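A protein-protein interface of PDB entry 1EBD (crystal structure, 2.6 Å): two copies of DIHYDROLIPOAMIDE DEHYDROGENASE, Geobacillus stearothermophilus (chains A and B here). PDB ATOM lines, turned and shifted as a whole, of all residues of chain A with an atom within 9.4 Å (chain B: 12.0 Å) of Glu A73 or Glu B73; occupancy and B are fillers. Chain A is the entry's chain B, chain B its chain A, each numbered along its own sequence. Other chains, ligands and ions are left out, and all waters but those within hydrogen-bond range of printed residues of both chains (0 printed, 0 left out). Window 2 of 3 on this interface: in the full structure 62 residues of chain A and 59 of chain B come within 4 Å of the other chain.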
ATOM      1  N   ALA A  62      -7.025  -1.840  12.033  1.00  0.00           N
ATOM      2  CA  ALA A  62      -7.860  -2.351  13.106  1.00  0.00           C
ATOM      3  C   ALA A  62      -8.856  -3.328  12.527  1.00  0.00           C
ATOM      4  O   ALA A  62      -8.906  -4.494  12.911  1.00  0.00           O
ATOM      5  CB  ALA A  62      -8.579  -1.217  13.791  1.00  0.00           C
ATOM      6  N   LYS A  63      -9.587  -2.866  11.527  1.00  0.00           N
ATOM      7  CA  LYS A  63     -10.584  -3.700  10.900  1.00  0.00           C
ATOM      8  C   LYS A  63     -10.034  -4.789   9.988  1.00  0.00           C
ATOM      9  O   LYS A  63     -10.791  -5.632   9.526  1.00  0.00           O
ATOM     10  CB  LYS A  63     -11.558  -2.828  10.120  1.00  0.00           C
ATOM     11  CG  LYS A  63     -12.260  -1.793  10.969  1.00  0.00           C
ATOM     12  CD  LYS A  63     -13.529  -1.301  10.289  1.00  0.00           C
ATOM     13  CE  LYS A  63     -14.672  -2.320  10.354  1.00  0.00           C
ATOM     14  NZ  LYS A  63     -15.236  -2.488  11.734  1.00  0.00           N
ATOM     15  N   HIS A  64      -8.734  -4.814   9.730  1.00  0.00           N
ATOM     16  CA  HIS A  64      -8.222  -5.831   8.814  1.00  0.00           C
ATOM     17  C   HIS A  64      -6.921  -6.560   9.141  1.00  0.00           C
ATOM     18  O   HIS A  64      -6.077  -6.739   8.262  1.00  0.00           O
ATOM     19  CB  HIS A  64      -8.138  -5.254   7.399  1.00  0.00           C
ATOM     20  CG  HIS A  64      -9.465  -4.876   6.826  1.00  0.00           C
ATOM     21  ND1 HIS A  64      -9.920  -3.571   6.804  1.00  0.00           N
ATOM     22  CD2 HIS A  64     -10.449  -5.624   6.273  1.00  0.00           C
ATOM     23  CE1 HIS A  64     -11.129  -3.537   6.259  1.00  0.00           C
ATOM     24  NE2 HIS A  64     -11.467  -4.770   5.932  1.00  0.00           N
ATOM     25  N   ILE A  70      -5.736 -11.418  14.587  1.00  0.00           N
ATOM     26  CA  ILE A  70      -6.315 -10.348  15.374  1.00  0.00           C
ATOM     27  C   ILE A  70      -7.693 -10.072  14.801  1.00  0.00           C
ATOM     28  O   ILE A  70      -7.835  -9.761  13.621  1.00  0.00           O
ATOM     29  CB  ILE A  70      -5.442  -9.097  15.309  1.00  0.00           C
ATOM     30  CG1 ILE A  70      -4.021  -9.452  15.729  1.00  0.00           C
ATOM     31  CG2 ILE A  70      -5.998  -8.017  16.217  1.00  0.00           C
ATOM     32  CD1 ILE A  70      -3.007  -8.464  15.266  1.00  0.00           C
ATOM     33  N   LYS A  71      -8.716 -10.239  15.624  1.00  0.00           N
ATOM     34  CA  LYS A  71     -10.077 -10.023  15.175  1.00  0.00           C
ATOM     35  C   LYS A  71     -10.826  -9.170  16.185  1.00  0.00           C
ATOM     36  O   LYS A  71     -11.090  -9.598  17.308  1.00  0.00           O
ATOM     37  CB  LYS A  71     -10.775 -11.371  14.982  1.00  0.00           C
ATOM     38  CG  LYS A  71      -9.938 -12.389  14.199  1.00  0.00           C
ATOM     39  CD  LYS A  71     -10.658 -13.719  13.992  1.00  0.00           C
ATOM     40  CE  LYS A  71      -9.746 -14.751  13.319  1.00  0.00           C
ATOM     41  NZ  LYS A  71      -9.200 -14.309  11.994  1.00  0.00           N
ATOM     42  N   ALA A  72     -11.103  -7.932  15.803  1.00  0.00           N
ATOM     43  CA  ALA A  72     -11.827  -7.008  16.666  1.00  0.00           C
ATOM     44  C   ALA A  72     -13.323  -7.213  16.447  1.00  0.00           C
ATOM     45  O   ALA A  72     -13.745  -8.230  15.890  1.00  0.00           O
ATOM     46  CB  ALA A  72     -11.432  -5.567  16.345  1.00  0.00           C
ATOM     47  N   GLU A  73     -14.119  -6.244  16.879  1.00  0.00           N
ATOM     48  CA  GLU A  73     -15.561  -6.302  16.720  1.00  0.00           C
ATOM     49  C   GLU A  73     -16.067  -4.889  16.937  1.00  0.00           C
ATOM     50  O   GLU A  73     -15.575  -4.184  17.813  1.00  0.00           O
ATOM     51  CB  GLU A  73     -16.173  -7.236  17.765  1.00  0.00           C
ATOM     52  CG  GLU A  73     -17.559  -7.747  17.398  1.00  0.00           C
ATOM     53  CD  GLU A  73     -18.542  -7.709  18.558  1.00  0.00           C
ATOM     54  OE1 GLU A  73     -18.133  -7.960  19.715  1.00  0.00           O
ATOM     55  OE2 GLU A  73     -19.734  -7.424  18.304  1.00  0.00           O
ATOM     56  N   ASN A  74     -17.003  -4.453  16.099  1.00  0.00           N
ATOM     57  CA  ASN A  74     -17.574  -3.110  16.209  1.00  0.00           C
ATOM     58  C   ASN A  74     -16.525  -2.006  16.383  1.00  0.00           C
ATOM     59  O   ASN A  74     -16.478  -1.358  17.433  1.00  0.00           O
ATOM     60  CB  ASN A  74     -18.571  -3.042  17.380  1.00  0.00           C
ATOM     61  CG  ASN A  74     -19.848  -3.830  17.126  1.00  0.00           C
ATOM     62  OD1 ASN A  74     -20.025  -4.437  16.065  1.00  0.00           O
ATOM     63  ND2 ASN A  74     -20.753  -3.818  18.102  1.00  0.00           N
ATOM     64  N   VAL A  75     -15.674  -1.805  15.378  1.00  0.00           N
ATOM     65  CA  VAL A  75     -14.658  -0.759  15.463  1.00  0.00           C
ATOM     66  C   VAL A  75     -15.280   0.555  15.011  1.00  0.00           C
ATOM     67  O   VAL A  75     -15.639   0.724  13.843  1.00  0.00           O
ATOM     68  CB  VAL A  75     -13.431  -1.062  14.601  1.00  0.00           C
ATOM     69  CG1 VAL A  75     -12.381   0.014  14.813  1.00  0.00           C
ATOM     70  CG2 VAL A  75     -12.864  -2.422  14.954  1.00  0.00           C
ATOM     71  N   THR A  76     -15.433   1.473  15.955  1.00  0.00           N
ATOM     72  CA  THR A  76     -16.035   2.760  15.679  1.00  0.00           C
ATOM     73  C   THR A  76     -15.039   3.862  15.381  1.00  0.00           C
ATOM     74  O   THR A  76     -13.935   3.892  15.930  1.00  0.00           O
ATOM     75  CB  THR A  76     -16.943   3.208  16.838  1.00  0.00           C
ATOM     76  OG1 THR A  76     -16.315   2.895  18.087  1.00  0.00           O
ATOM     77  CG2 THR A  76     -18.281   2.508  16.765  1.00  0.00           C
ATOM     78  N   ILE A  77     -15.434   4.733  14.460  1.00  0.00           N
ATOM     79  CA  ILE A  77     -14.641   5.887  14.059  1.00  0.00           C
ATOM     80  C   ILE A  77     -15.455   7.115  14.424  1.00  0.00           C
ATOM     81  O   ILE A  77     -16.650   7.191  14.142  1.00  0.00           O
ATOM     82  CB  ILE A  77     -14.303   5.899  12.531  1.00  0.00           C
ATOM     83  CG1 ILE A  77     -13.669   7.230  12.144  1.00  0.00           C
ATOM     84  CG2 ILE A  77     -15.528   5.664  11.685  1.00  0.00           C
ATOM     85  CD1 ILE A  77     -12.294   7.423  12.720  1.00  0.00           C
ATOM     86  N   ARG B  58       0.344  -5.036  16.218  1.00  0.00           N
ATOM     87  CA  ARG B  58      -0.901  -4.873  15.479  1.00  0.00           C
ATOM     88  C   ARG B  58      -2.008  -4.930  16.526  1.00  0.00           C
ATOM     89  O   ARG B  58      -3.056  -4.305  16.370  1.00  0.00           O
ATOM     90  CB  ARG B  58      -1.108  -6.014  14.487  1.00  0.00           C
ATOM     91  CG  ARG B  58      -0.221  -5.969  13.284  1.00  0.00           C
ATOM     92  CD  ARG B  58      -0.586  -4.811  12.405  1.00  0.00           C
ATOM     93  NE  ARG B  58       0.137  -4.861  11.141  1.00  0.00           N
ATOM     94  CZ  ARG B  58      -0.346  -5.390  10.020  1.00  0.00           C
ATOM     95  NH1 ARG B  58      -1.564  -5.924   9.999  1.00  0.00           N
ATOM     96  NH2 ARG B  58       0.387  -5.367   8.912  1.00  0.00           N
ATOM     97  N   TYR B  59      -1.752  -5.685  17.594  1.00  0.00           N
ATOM     98  CA  TYR B  59      -2.685  -5.849  18.704  1.00  0.00           C
ATOM     99  C   TYR B  59      -2.668  -4.612  19.623  1.00  0.00           C
ATOM    100  O   TYR B  59      -3.727  -4.112  19.997  1.00  0.00           O
ATOM    101  CB  TYR B  59      -2.340  -7.118  19.487  1.00  0.00           C
ATOM    102  CG  TYR B  59      -3.378  -7.507  20.511  1.00  0.00           C
ATOM    103  CD1 TYR B  59      -4.476  -8.279  20.152  1.00  0.00           C
ATOM    104  CD2 TYR B  59      -3.266  -7.097  21.840  1.00  0.00           C
ATOM    105  CE1 TYR B  59      -5.441  -8.636  21.089  1.00  0.00           C
ATOM    106  CE2 TYR B  59      -4.224  -7.447  22.785  1.00  0.00           C
ATOM    107  CZ  TYR B  59      -5.308  -8.215  22.403  1.00  0.00           C
ATOM    108  OH  TYR B  59      -6.268  -8.561  23.324  1.00  0.00           O
ATOM    109  N   GLU B  60      -1.473  -4.133  19.985  1.00  0.00           N
ATOM    110  CA  GLU B  60      -1.311  -2.937  20.828  1.00  0.00           C
ATOM    111  C   GLU B  60      -2.116  -1.805  20.183  1.00  0.00           C
ATOM    112  O   GLU B  60      -2.976  -1.194  20.820  1.00  0.00           O
ATOM    113  CB  GLU B  60       0.192  -2.561  20.925  1.00  0.00           C
ATOM    114  CG  GLU B  60       0.590  -1.114  21.388  1.00  0.00           C
ATOM    115  CD  GLU B  60       2.136  -0.902  21.447  1.00  0.00           C
ATOM    116  OE1 GLU B  60       2.826  -1.930  21.571  1.00  0.00           O
ATOM    117  OE2 GLU B  60       2.688   0.245  21.373  1.00  0.00           O
ATOM    118  N   GLN B  61      -1.914  -1.627  18.880  1.00  0.00           N
ATOM    119  CA  GLN B  61      -2.571  -0.575  18.121  1.00  0.00           C
ATOM    120  C   GLN B  61      -4.065  -0.668  17.942  1.00  0.00           C
ATOM    121  O   GLN B  61      -4.764   0.325  18.132  1.00  0.00           O
ATOM    122  CB  GLN B  61      -1.901  -0.397  16.771  1.00  0.00           C
ATOM    123  CG  GLN B  61      -0.490   0.080  16.911  1.00  0.00           C
ATOM    124  CD  GLN B  61      -0.033   0.867  15.721  1.00  0.00           C
ATOM    125  OE1 GLN B  61      -0.097   0.395  14.586  1.00  0.00           O
ATOM    126  NE2 GLN B  61       0.429   2.086  15.965  1.00  0.00           N
ATOM    127  N   ALA B  62      -4.560  -1.831  17.539  1.00  0.00           N
ATOM    128  CA  ALA B  62      -5.999  -1.999  17.347  1.00  0.00           C
ATOM    129  C   ALA B  62      -6.720  -1.610  18.629  1.00  0.00           C
ATOM    130  O   ALA B  62      -7.660  -0.815  18.631  1.00  0.00           O
ATOM    131  CB  ALA B  62      -6.312  -3.442  17.006  1.00  0.00           C
ATOM    132  N   LYS B  63      -6.170  -2.107  19.726  1.00  0.00           N
ATOM    133  CA  LYS B  63      -6.690  -1.922  21.068  1.00  0.00           C
ATOM    134  C   LYS B  63      -6.438  -0.551  21.713  1.00  0.00           C
ATOM    135  O   LYS B  63      -7.093  -0.215  22.699  1.00  0.00           O
ATOM    136  CB  LYS B  63      -6.075  -3.018  21.935  1.00  0.00           C
ATOM    137  CG  LYS B  63      -6.896  -3.537  23.085  1.00  0.00           C
ATOM    138  CD  LYS B  63      -6.053  -4.572  23.814  1.00  0.00           C
ATOM    139  CE  LYS B  63      -6.690  -5.058  25.095  1.00  0.00           C
ATOM    140  NZ  LYS B  63      -5.697  -5.847  25.889  1.00  0.00           N
ATOM    141  N   HIS B  64      -5.496   0.237  21.203  1.00  0.00           N
ATOM    142  CA  HIS B  64      -5.223   1.530  21.833  1.00  0.00           C
ATOM    143  C   HIS B  64      -5.058   2.774  20.949  1.00  0.00           C
ATOM    144  O   HIS B  64      -4.226   3.635  21.240  1.00  0.00           O
ATOM    145  CB  HIS B  64      -4.031   1.408  22.796  1.00  0.00           C
ATOM    146  CG  HIS B  64      -4.318   0.605  24.032  1.00  0.00           C
ATOM    147  ND1 HIS B  64      -3.732  -0.622  24.277  1.00  0.00           N
ATOM    148  CD2 HIS B  64      -5.114   0.854  25.100  1.00  0.00           C
ATOM    149  CE1 HIS B  64      -4.156  -1.089  25.443  1.00  0.00           C
ATOM    150  NE2 HIS B  64      -4.995  -0.211  25.958  1.00  0.00           N
ATOM    151  N   SER B  65      -5.901   2.914  19.925  1.00  0.00           N
ATOM    152  CA  SER B  65      -5.859   4.081  19.031  1.00  0.00           C
ATOM    153  C   SER B  65      -6.957   5.065  19.445  1.00  0.00           C
ATOM    154  O   SER B  65      -7.418   5.899  18.660  1.00  0.00           O
ATOM    155  CB  SER B  65      -6.067   3.635  17.589  1.00  0.00           C
ATOM    156  OG  SER B  65      -5.052   2.726  17.209  1.00  0.00           O
ATOM    157  N   GLU B  66      -7.333   4.954  20.714  1.00  0.00           N
ATOM    158  CA  GLU B  66      -8.365   5.747  21.378  1.00  0.00           C
ATOM    159  C   GLU B  66      -8.281   7.244  21.064  1.00  0.00           C
ATOM    160  O   GLU B  66      -9.233   7.841  20.566  1.00  0.00           O
ATOM    161  CB  GLU B  66      -8.251   5.511  22.904  1.00  0.00           C
ATOM    162  CG  GLU B  66      -8.234   4.005  23.335  1.00  0.00           C
ATOM    163  CD  GLU B  66      -7.125   3.615  24.348  1.00  0.00           C
ATOM    164  OE1 GLU B  66      -6.034   4.234  24.365  1.00  0.00           O
ATOM    165  OE2 GLU B  66      -7.344   2.652  25.118  1.00  0.00           O
ATOM    166  N   GLY B  69      -9.472   8.731  17.979  1.00  0.00           N
ATOM    167  CA  GLY B  69     -10.886   8.592  17.712  1.00  0.00           C
ATOM    168  C   GLY B  69     -11.312   7.279  17.098  1.00  0.00           C
ATOM    169  O   GLY B  69     -12.375   7.214  16.486  1.00  0.00           O
ATOM    170  N   ILE B  70     -10.476   6.252  17.192  1.00  0.00           N
ATOM    171  CA  ILE B  70     -10.854   4.940  16.677  1.00  0.00           C
ATOM    172  C   ILE B  70     -11.057   4.085  17.915  1.00  0.00           C
ATOM    173  O   ILE B  70     -10.121   3.872  18.682  1.00  0.00           O
ATOM    174  CB  ILE B  70      -9.760   4.286  15.795  1.00  0.00           C
ATOM    175  CG1 ILE B  70      -9.528   5.098  14.521  1.00  0.00           C
ATOM    176  CG2 ILE B  70     -10.175   2.871  15.408  1.00  0.00           C
ATOM    177  CD1 ILE B  70      -8.644   6.296  14.711  1.00  0.00           C
ATOM    178  N   LYS B  71     -12.282   3.633  18.140  1.00  0.00           N
ATOM    179  CA  LYS B  71     -12.574   2.819  19.310  1.00  0.00           C
ATOM    180  C   LYS B  71     -12.927   1.402  18.909  1.00  0.00           C
ATOM    181  O   LYS B  71     -13.991   1.156  18.364  1.00  0.00           O
ATOM    182  CB  LYS B  71     -13.730   3.420  20.126  1.00  0.00           C
ATOM    183  CG  LYS B  71     -13.460   4.782  20.805  1.00  0.00           C
ATOM    184  CD  LYS B  71     -13.411   5.959  19.808  1.00  0.00           C
ATOM    185  CE  LYS B  71     -14.057   7.249  20.359  1.00  0.00           C
ATOM    186  NZ  LYS B  71     -13.416   7.823  21.584  1.00  0.00           N
ATOM    187  N   ALA B  72     -12.005   0.478  19.131  1.00  0.00           N
ATOM    188  CA  ALA B  72     -12.244  -0.922  18.812  1.00  0.00           C
ATOM    189  C   ALA B  72     -12.807  -1.552  20.072  1.00  0.00           C
ATOM    190  O   ALA B  72     -12.297  -1.315  21.170  1.00  0.00           O
ATOM    191  CB  ALA B  72     -10.947  -1.611  18.411  1.00  0.00           C
ATOM    192  N   GLU B  73     -13.878  -2.319  19.925  1.00  0.00           N
ATOM    193  CA  GLU B  73     -14.491  -2.954  21.072  1.00  0.00           C
ATOM    194  C   GLU B  73     -14.278  -4.446  21.006  1.00  0.00           C
ATOM    195  O   GLU B  73     -14.643  -5.084  20.027  1.00  0.00           O
ATOM    196  CB  GLU B  73     -15.985  -2.641  21.120  1.00  0.00           C
ATOM    197  CG  GLU B  73     -16.555  -2.624  22.529  1.00  0.00           C
ATOM    198  CD  GLU B  73     -15.969  -1.506  23.386  1.00  0.00           C
ATOM    199  OE1 GLU B  73     -14.832  -1.661  23.888  1.00  0.00           O
ATOM    200  OE2 GLU B  73     -16.650  -0.470  23.558  1.00  0.00           O
ATOM    201  N   ASN B  74     -13.655  -4.996  22.041  1.00  0.00           N
ATOM    202  CA  ASN B  74     -13.403  -6.429  22.100  1.00  0.00           C
ATOM    203  C   ASN B  74     -12.446  -6.875  20.983  1.00  0.00           C
ATOM    204  O   ASN B  74     -12.876  -7.346  19.925  1.00  0.00           O
ATOM    205  CB  ASN B  74     -14.743  -7.194  22.036  1.00  0.00           C
ATOM    206  CG  ASN B  74     -14.566  -8.705  21.992  1.00  0.00           C
ATOM    207  OD1 ASN B  74     -14.271  -9.340  23.004  1.00  0.00           O
ATOM    208  ND2 ASN B  74     -14.755  -9.287  20.816  1.00  0.00           N
ATOM    209  N   VAL B  75     -11.148  -6.670  21.208  1.00  0.00           N
ATOM    210  CA  VAL B  75     -10.124  -7.069  20.242  1.00  0.00           C
ATOM    211  C   VAL B  75      -9.615  -8.453  20.650  1.00  0.00           C
ATOM    212  O   VAL B  75      -9.069  -8.634  21.744  1.00  0.00           O
ATOM    213  CB  VAL B  75      -8.942  -6.070  20.196  1.00  0.00           C
ATOM    214  CG1 VAL B  75      -7.937  -6.495  19.138  1.00  0.00           C
ATOM    215  CG2 VAL B  75      -9.443  -4.680  19.888  1.00  0.00           C
ATOM    216  N   THR B  76      -9.834  -9.429  19.776  1.00  0.00           N
ATOM    217  CA  THR B  76      -9.434 -10.806  20.027  1.00  0.00           C
ATOM    218  C   THR B  76      -8.149 -11.189  19.295  1.00  0.00           C
ATOM    219  O   THR B  76      -7.772 -10.559  18.306  1.00  0.00           O
ATOM    220  CB  THR B  76     -10.598 -11.770  19.662  1.00  0.00           C
ATOM    221  OG1 THR B  76     -10.984 -12.514  20.825  1.00  0.00           O
ATOM    222  CG2 THR B  76     -10.219 -12.732  18.522  1.00  0.00           C
ATOM    223  N   ILE B  77      -7.488 -12.232  19.782  1.00  0.00           N
ATOM    224  CA  ILE B  77      -6.252 -12.699  19.183  1.00  0.00           C
ATOM    225  C   ILE B  77      -6.213 -14.234  19.165  1.00  0.00           C
ATOM    226  O   ILE B  77      -6.176 -14.878  20.215  1.00  0.00           O
ATOM    227  CB  ILE B  77      -5.018 -12.108  19.940  1.00  0.00           C
ATOM    228  CG1 ILE B  77      -3.705 -12.605  19.339  1.00  0.00           C
ATOM    229  CG2 ILE B  77      -5.089 -12.414  21.421  1.00  0.00           C
ATOM    230  CD1 ILE B  77      -3.312 -11.891  18.081  1.00  0.00           C
ATOM    231  N   ASP B  78      -6.297 -14.813  17.970  1.00  0.00           N
ATOM    232  CA  ASP B  78      -6.252 -16.262  17.792  1.00  0.00           C
ATOM    233  C   ASP B  78      -4.773 -16.629  17.686  1.00  0.00           C
ATOM    234  O   ASP B  78      -4.210 -16.710  16.588  1.00  0.00           O
ATOM    235  CB  ASP B  78      -7.016 -16.676  16.516  1.00  0.00           C
ATOM    236  CG  ASP B  78      -7.119 -18.201  16.331  1.00  0.00           C
ATOM    237  OD1 ASP B  78      -6.611 -18.968  17.178  1.00  0.00           O
ATOM    238  OD2 ASP B  78      -7.715 -18.638  15.322  1.00  0.00           O
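The side-chain hydroxyl of Tyr B59 is in hydrogen-bond range of the backbone carbonyl oxygen of Val B75. The backbone NH (N) of Ile B70 is in hydrogen-bond range of the backbone carbonyl oxygen (O) of Ser B65, at 3.4 Å.
Among the printed residues, pairs that only touch across the chains: Ile A70 with Arg B58, Ile A70 with Thr B76, Thr A76 with Ile B70, Ala A72 with Asn B74, Ile A70 with Ile B77, Val A75 with Lys B71, Ile A77 with Gly B69, Asn A74 with Lys B71, Val A75 with Ile B70, Thr A76 with Gly B69, Asn A74 with Glu B73, Ile A70 with Val B75, Lys A71 with Val B75, Ile A70 with Tyr B59, Lys A71 with Asn B74 and Ala A72 with Val B75.
The backbone NH (N) of Lys B71 sits at hydrogen-bond distance from the backbone carbonyl oxygen (O) of Thr A76, at 2.8 Å. N of Glu B73 lies within hydrogen-bond range of O of Glu A73, at 3.3 Å. The backbone NH (N) of Glu A73 sits at hydrogen-bond distance from the backbone carbonyl oxygen (O) of Asn B74, at 3.5 Å. N of Thr B76 lies within hydrogen-bond range of O of Lys A71.
Of the printed residues of chain B, Lys A71 touches Asn B74 (3.9 Å), Val B75 (3.8 Å) and Thr B76 (2.8 Å). Printed residues of chain B within 4 Å of Glu A73: Glu B73 (2.6 Å) and Asn B74 (3.5 Å). Of chain B, only Ile B70 (3.7 Å) and Lys B71 (3.5 Å) come within 4 Å of Val A75. Of the printed residues of chain B, Ile A77 touches Gly B69. Printed residues of chain A within 4 Å of Arg B58: Ile A70. Printed residues of chain A within 4 Å of Ile B70: Val A75 (3.7 Å) and Thr A76 (3.3 Å). No residue of chain A comes within 4 Å of Ala B72. Printed residues of chain A within 4 Å of Glu B73: Glu A73 (2.6 Å) and Asn A74 (3.7 Å). Asn B74 touches just these residues of chain A: Lys A71 (3.9 Å), Ala A72 (3.4 Å) and Glu A73 (3.5 Å). Of the printed residues of chain A, Val B75 touches Ile A70 (3.8 Å), Lys A71 (3.8 Å) and Ala A72 (3.96 Å). The nearest residue of chain A that does not touch Glu B73 is Ala A72 (4.4 Å).
Ile A70 touches Thr B76, and with the chains exchanged Thr A76 touches Ile B70. Ala A72 touches Asn B74, but with the chains exchanged Asn A74 does not touch Ala B72 (4.5 Å). Glu A73 touches its own counterpart, Glu B73. Glu A73 touches Asn B74, and with the chains exchanged Asn A74 touches Glu B73. 11 positions are printed for both chains.
Hydrophobic or aromatic side chains of chain A within 4 Å of the printed part of chain B: Ile A70, Val A75 and Ile A77. Printed residues of chain B that touch a printed residue of chain A: Arg B58, Tyr B59, Gly B69, Ile B70, Lys B71, Glu B73, Asn B74, Val B75, Thr B76 and Ile B77.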
